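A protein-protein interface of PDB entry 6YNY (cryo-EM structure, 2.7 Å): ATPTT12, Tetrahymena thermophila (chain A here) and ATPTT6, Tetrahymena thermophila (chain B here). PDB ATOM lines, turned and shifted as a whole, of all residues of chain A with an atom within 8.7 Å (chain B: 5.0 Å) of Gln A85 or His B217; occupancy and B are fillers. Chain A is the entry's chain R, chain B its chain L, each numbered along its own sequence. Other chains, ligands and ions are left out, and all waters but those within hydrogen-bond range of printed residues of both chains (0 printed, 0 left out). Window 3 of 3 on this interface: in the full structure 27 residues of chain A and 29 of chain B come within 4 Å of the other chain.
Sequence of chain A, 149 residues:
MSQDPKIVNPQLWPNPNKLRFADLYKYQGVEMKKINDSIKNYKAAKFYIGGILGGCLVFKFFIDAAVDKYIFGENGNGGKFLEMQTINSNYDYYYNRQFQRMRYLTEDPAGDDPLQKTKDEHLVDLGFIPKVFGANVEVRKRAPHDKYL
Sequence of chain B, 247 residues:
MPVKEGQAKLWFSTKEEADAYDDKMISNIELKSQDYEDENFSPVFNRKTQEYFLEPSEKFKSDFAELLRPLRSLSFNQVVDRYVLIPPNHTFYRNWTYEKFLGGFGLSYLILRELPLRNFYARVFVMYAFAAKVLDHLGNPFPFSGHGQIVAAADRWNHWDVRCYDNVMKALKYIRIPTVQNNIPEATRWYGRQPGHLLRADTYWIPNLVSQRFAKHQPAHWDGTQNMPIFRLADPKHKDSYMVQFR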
ATOM      1  N   LYS A  80      15.585 -14.428  10.428  1.00  0.00           N
ATOM      2  CA  LYS A  80      16.576 -15.338   9.876  1.00  0.00           C
ATOM      3  C   LYS A  80      17.028 -16.390  10.874  1.00  0.00           C
ATOM      4  O   LYS A  80      17.739 -17.322  10.486  1.00  0.00           O
ATOM      5  CB  LYS A  80      17.779 -14.546   9.379  1.00  0.00           C
ATOM      6  CG  LYS A  80      17.447 -13.601   8.257  1.00  0.00           C
ATOM      7  CD  LYS A  80      18.686 -12.928   7.718  1.00  0.00           C
ATOM      8  CE  LYS A  80      18.334 -11.912   6.653  1.00  0.00           C
ATOM      9  NZ  LYS A  80      19.541 -11.275   6.071  1.00  0.00           N
ATOM     10  N   LEU A  82      15.274 -18.621  11.981  1.00  0.00           N
ATOM     11  CA  LEU A  82      14.596 -19.837  11.561  1.00  0.00           C
ATOM     12  C   LEU A  82      15.151 -20.419  10.271  1.00  0.00           C
ATOM     13  O   LEU A  82      14.723 -21.503   9.866  1.00  0.00           O
ATOM     14  CB  LEU A  82      13.104 -19.559  11.377  1.00  0.00           C
ATOM     15  CG  LEU A  82      12.371 -19.029  12.605  1.00  0.00           C
ATOM     16  CD1 LEU A  82      10.992 -18.565  12.218  1.00  0.00           C
ATOM     17  CD2 LEU A  82      12.293 -20.094  13.672  1.00  0.00           C
ATOM     18  N   GLU A  83      16.082 -19.734   9.616  1.00  0.00           N
ATOM     19  CA  GLU A  83      16.631 -20.198   8.354  1.00  0.00           C
ATOM     20  C   GLU A  83      17.808 -21.129   8.593  1.00  0.00           C
ATOM     21  O   GLU A  83      18.674 -20.857   9.428  1.00  0.00           O
ATOM     22  CB  GLU A  83      17.075 -19.017   7.492  1.00  0.00           C
ATOM     23  CG  GLU A  83      15.967 -18.047   7.167  1.00  0.00           C
ATOM     24  CD  GLU A  83      16.451 -16.867   6.358  1.00  0.00           C
ATOM     25  OE1 GLU A  83      17.640 -16.854   5.981  1.00  0.00           O
ATOM     26  OE2 GLU A  83      15.643 -15.951   6.097  1.00  0.00           O
ATOM     27  N   MET A  84      17.829 -22.233   7.854  1.00  0.00           N
ATOM     28  CA  MET A  84      18.931 -23.179   7.892  1.00  0.00           C
ATOM     29  C   MET A  84      19.203 -23.652   6.476  1.00  0.00           C
ATOM     30  O   MET A  84      18.277 -24.038   5.758  1.00  0.00           O
ATOM     31  CB  MET A  84      18.618 -24.361   8.812  1.00  0.00           C
ATOM     32  CG  MET A  84      17.349 -25.081   8.469  1.00  0.00           C
ATOM     33  SD  MET A  84      16.917 -26.331   9.678  1.00  0.00           S
ATOM     34  CE  MET A  84      15.369 -26.873   8.995  1.00  0.00           C
ATOM     35  N   GLN A  85      20.469 -23.611   6.078  1.00  0.00           N
ATOM     36  CA  GLN A  85      20.881 -23.923   4.722  1.00  0.00           C
ATOM     37  C   GLN A  85      21.933 -25.022   4.740  1.00  0.00           C
ATOM     38  O   GLN A  85      22.590 -25.268   5.754  1.00  0.00           O
ATOM     39  CB  GLN A  85      21.416 -22.671   4.016  1.00  0.00           C
ATOM     40  CG  GLN A  85      22.365 -21.842   4.848  1.00  0.00           C
ATOM     41  CD  GLN A  85      22.767 -20.561   4.160  1.00  0.00           C
ATOM     42  OE1 GLN A  85      22.182 -20.175   3.149  1.00  0.00           O
ATOM     43  NE2 GLN A  85      23.772 -19.891   4.704  1.00  0.00           N
ATOM     44  N   THR A  86      22.084 -25.689   3.598  1.00  0.00           N
ATOM     45  CA  THR A  86      22.983 -26.824   3.484  1.00  0.00           C
ATOM     46  C   THR A  86      23.655 -26.831   2.121  1.00  0.00           C
ATOM     47  O   THR A  86      23.203 -26.184   1.174  1.00  0.00           O
ATOM     48  CB  THR A  86      22.246 -28.151   3.695  1.00  0.00           C
ATOM     49  OG1 THR A  86      23.169 -29.240   3.576  1.00  0.00           O
ATOM     50  CG2 THR A  86      21.143 -28.320   2.676  1.00  0.00           C
ATOM     51  N   ILE A  87      24.753 -27.585   2.040  1.00  0.00           N
ATOM     52  CA  ILE A  87      25.476 -27.784   0.792  1.00  0.00           C
ATOM     53  C   ILE A  87      25.205 -29.149   0.185  1.00  0.00           C
ATOM     54  O   ILE A  87      25.770 -29.474  -0.867  1.00  0.00           O
ATOM     55  CB  ILE A  87      26.990 -27.593   0.998  1.00  0.00           C
ATOM     56  CG1 ILE A  87      27.553 -28.683   1.903  1.00  0.00           C
ATOM     57  CG2 ILE A  87      27.260 -26.246   1.608  1.00  0.00           C
ATOM     58  CD1 ILE A  87      29.030 -28.575   2.138  1.00  0.00           C
ATOM     59  N   ASN A  88      24.369 -29.961   0.818  1.00  0.00           N
ATOM     60  CA  ASN A  88      24.072 -31.285   0.299  1.00  0.00           C
ATOM     61  C   ASN A  88      23.270 -31.199  -0.987  1.00  0.00           C
ATOM     62  O   ASN A  88      22.405 -30.335  -1.147  1.00  0.00           O
ATOM     63  CB  ASN A  88      23.294 -32.097   1.327  1.00  0.00           C
ATOM     64  CG  ASN A  88      24.147 -32.553   2.472  1.00  0.00           C
ATOM     65  OD1 ASN A  88      25.294 -32.137   2.618  1.00  0.00           O
ATOM     66  ND2 ASN A  88      23.591 -33.415   3.300  1.00  0.00           N
ATOM     67  N   GLN B 212      34.845 -27.289  -0.571  1.00  0.00           N
ATOM     68  CA  GLN B 212      33.807 -26.540   0.125  1.00  0.00           C
ATOM     69  C   GLN B 212      33.916 -25.039  -0.088  1.00  0.00           C
ATOM     70  O   GLN B 212      33.008 -24.307   0.319  1.00  0.00           O
ATOM     71  CB  GLN B 212      33.843 -26.860   1.616  1.00  0.00           C
ATOM     72  CG  GLN B 212      33.466 -28.289   1.934  1.00  0.00           C
ATOM     73  CD  GLN B 212      33.396 -28.558   3.414  1.00  0.00           C
ATOM     74  OE1 GLN B 212      33.960 -27.822   4.221  1.00  0.00           O
ATOM     75  NE2 GLN B 212      32.694 -29.616   3.784  1.00  0.00           N
ATOM     76  N   ALA B 215      31.356 -24.605  -2.876  1.00  0.00           N
ATOM     77  CA  ALA B 215      30.040 -25.153  -2.597  1.00  0.00           C
ATOM     78  C   ALA B 215      29.035 -24.037  -2.352  1.00  0.00           C
ATOM     79  O   ALA B 215      29.361 -22.986  -1.794  1.00  0.00           O
ATOM     80  CB  ALA B 215      30.095 -26.076  -1.384  1.00  0.00           C
ATOM     81  N   LYS B 216      27.799 -24.276  -2.779  1.00  0.00           N
ATOM     82  CA  LYS B 216      26.721 -23.308  -2.645  1.00  0.00           C
ATOM     83  C   LYS B 216      25.802 -23.734  -1.510  1.00  0.00           C
ATOM     84  O   LYS B 216      25.201 -24.812  -1.562  1.00  0.00           O
ATOM     85  CB  LYS B 216      25.938 -23.183  -3.949  1.00  0.00           C
ATOM     86  CG  LYS B 216      26.789 -22.780  -5.131  1.00  0.00           C
ATOM     87  CD  LYS B 216      25.937 -22.281  -6.285  1.00  0.00           C
ATOM     88  CE  LYS B 216      26.787 -21.890  -7.482  1.00  0.00           C
ATOM     89  NZ  LYS B 216      27.858 -20.920  -7.117  1.00  0.00           N
ATOM     90  N   HIS B 217      25.699 -22.890  -0.489  1.00  0.00           N
ATOM     91  CA  HIS B 217      24.816 -23.150   0.641  1.00  0.00           C
ATOM     92  C   HIS B 217      23.396 -22.774   0.248  1.00  0.00           C
ATOM     93  O   HIS B 217      23.063 -21.589   0.148  1.00  0.00           O
ATOM     94  CB  HIS B 217      25.270 -22.368   1.867  1.00  0.00           C
ATOM     95  CG  HIS B 217      26.576 -22.831   2.427  1.00  0.00           C
ATOM     96  ND1 HIS B 217      27.783 -22.564   1.822  1.00  0.00           N
ATOM     97  CD2 HIS B 217      26.860 -23.550   3.536  1.00  0.00           C
ATOM     98  CE1 HIS B 217      28.757 -23.097   2.536  1.00  0.00           C
ATOM     99  NE2 HIS B 217      28.224 -23.700   3.582  1.00  0.00           N
ATOM    100  N   GLN B 218      22.576 -23.761   0.026  1.00  0.00           N
ATOM    101  CA  GLN B 218      21.202 -23.529  -0.365  1.00  0.00           C
ATOM    102  C   GLN B 218      20.275 -23.687   0.832  1.00  0.00           C
ATOM    103  O   GLN B 218      20.572 -24.442   1.762  1.00  0.00           O
ATOM    104  CB  GLN B 218      20.779 -24.502  -1.466  1.00  0.00           C
ATOM    105  CG  GLN B 218      21.603 -24.399  -2.727  1.00  0.00           C
ATOM    106  CD  GLN B 218      21.508 -23.033  -3.370  1.00  0.00           C
ATOM    107  OE1 GLN B 218      20.563 -22.284  -3.125  1.00  0.00           O
ATOM    108  NE2 GLN B 218      22.491 -22.698  -4.195  1.00  0.00           N
ATOM    109  N   PRO B 219      19.146 -22.983   0.839  1.00  0.00           N
ATOM    110  CA  PRO B 219      18.226 -23.085   1.976  1.00  0.00           C
ATOM    111  C   PRO B 219      17.625 -24.478   2.083  1.00  0.00           C
ATOM    112  O   PRO B 219      17.177 -25.055   1.092  1.00  0.00           O
ATOM    113  CB  PRO B 219      17.160 -22.031   1.663  1.00  0.00           C
ATOM    114  CG  PRO B 219      17.222 -21.856   0.200  1.00  0.00           C
ATOM    115  CD  PRO B 219      18.646 -22.056  -0.187  1.00  0.00           C
ATOM    116  N   ALA B 220      17.628 -25.014   3.298  1.00  0.00           N
ATOM    117  CA  ALA B 220      17.020 -26.306   3.598  1.00  0.00           C
ATOM    118  C   ALA B 220      15.633 -26.036   4.162  1.00  0.00           C
ATOM    119  O   ALA B 220      15.482 -25.710   5.341  1.00  0.00           O
ATOM    120  CB  ALA B 220      17.879 -27.103   4.572  1.00  0.00           C
ATOM    121  N   PHE B 231      23.046 -32.296   7.122  1.00  0.00           N
ATOM    122  CA  PHE B 231      24.481 -32.496   7.202  1.00  0.00           C
ATOM    123  C   PHE B 231      24.768 -33.978   6.991  1.00  0.00           C
ATOM    124  O   PHE B 231      23.878 -34.765   6.664  1.00  0.00           O
ATOM    125  CB  PHE B 231      25.039 -32.019   8.543  1.00  0.00           C
ATOM    126  CG  PHE B 231      24.529 -30.685   8.976  1.00  0.00           C
ATOM    127  CD1 PHE B 231      24.771 -29.556   8.223  1.00  0.00           C
ATOM    128  CD2 PHE B 231      23.823 -30.556  10.154  1.00  0.00           C
ATOM    129  CE1 PHE B 231      24.304 -28.332   8.630  1.00  0.00           C
ATOM    130  CE2 PHE B 231      23.358 -29.336  10.563  1.00  0.00           C
ATOM    131  CZ  PHE B 231      23.598 -28.224   9.802  1.00  0.00           C
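The backbone carbonyl oxygen (O) of Gln B218 lies within hydrogen-bond range of the backbone NH (N) of Thr A86, at 2.7 Å.
The backbone carbonyl oxygen (O) of His B217 sits close to the side-chain amide oxygen (OE1) of Gln A85.
N of Ala B220 lies within hydrogen-bond range of O of Met A84, at 2.7 Å.
OG1 of Thr A86 lies within hydrogen-bond range of N of Asn A88, at 3.1 Å.
Among the printed residues, pairs that only touch across the chains: Met A84 with Pro B219 (3.8 Å), Gln A85 with Gln B218 (3.0 Å), Gln A85 with Pro B219 (3.8 Å), Gln A85 with Ala B220 (3.7 Å), Thr A86 with Lys B216 (3.7 Å), Thr A86 with His B217 (3.5 Å), Thr A86 with Ala B220 (3.97 Å), Ile A87 with Lys B216 (3.8 Å), Ile A87 with His B217 (3.3 Å) and Asn A88 with Phe B231 (3.6 Å).
His B217 touches just these residues of chain A: Gln A85 (3.4 Å), Thr A86 (3.5 Å) and Ile A87 (3.3 Å).
Of the printed residues of chain A, Phe B231 touches Asn A88 (3.6 Å).
Printed residues of chain A within 4 Å of Pro B219: Met A84 (3.8 Å) and Gln A85 (3.8 Å).
Ala B215 touches none of the printed residues of chain A.
Lys A80 touches none of the printed residues of chain B.
The nearest residue of chain B that does not touch Gln A85 is Phe B231 (4.5 Å).
Of the 8 printed residues of chain B, 6 touch a printed residue of chain A.
Printed residues of chain B that touch a printed residue of chain A: Lys B216, His B217, Gln B218, Pro B219, Ala B220 and Phe B231.
Of the 8 printed residues of chain A, 5 touch a printed residue of chain B.
Among the printed residues, 13 pairs touch across the chains.
Among the printed residues, no Asp or Glu carboxylate lies within 4 Å of a Lys or Arg side-chain nitrogen of the other chain.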
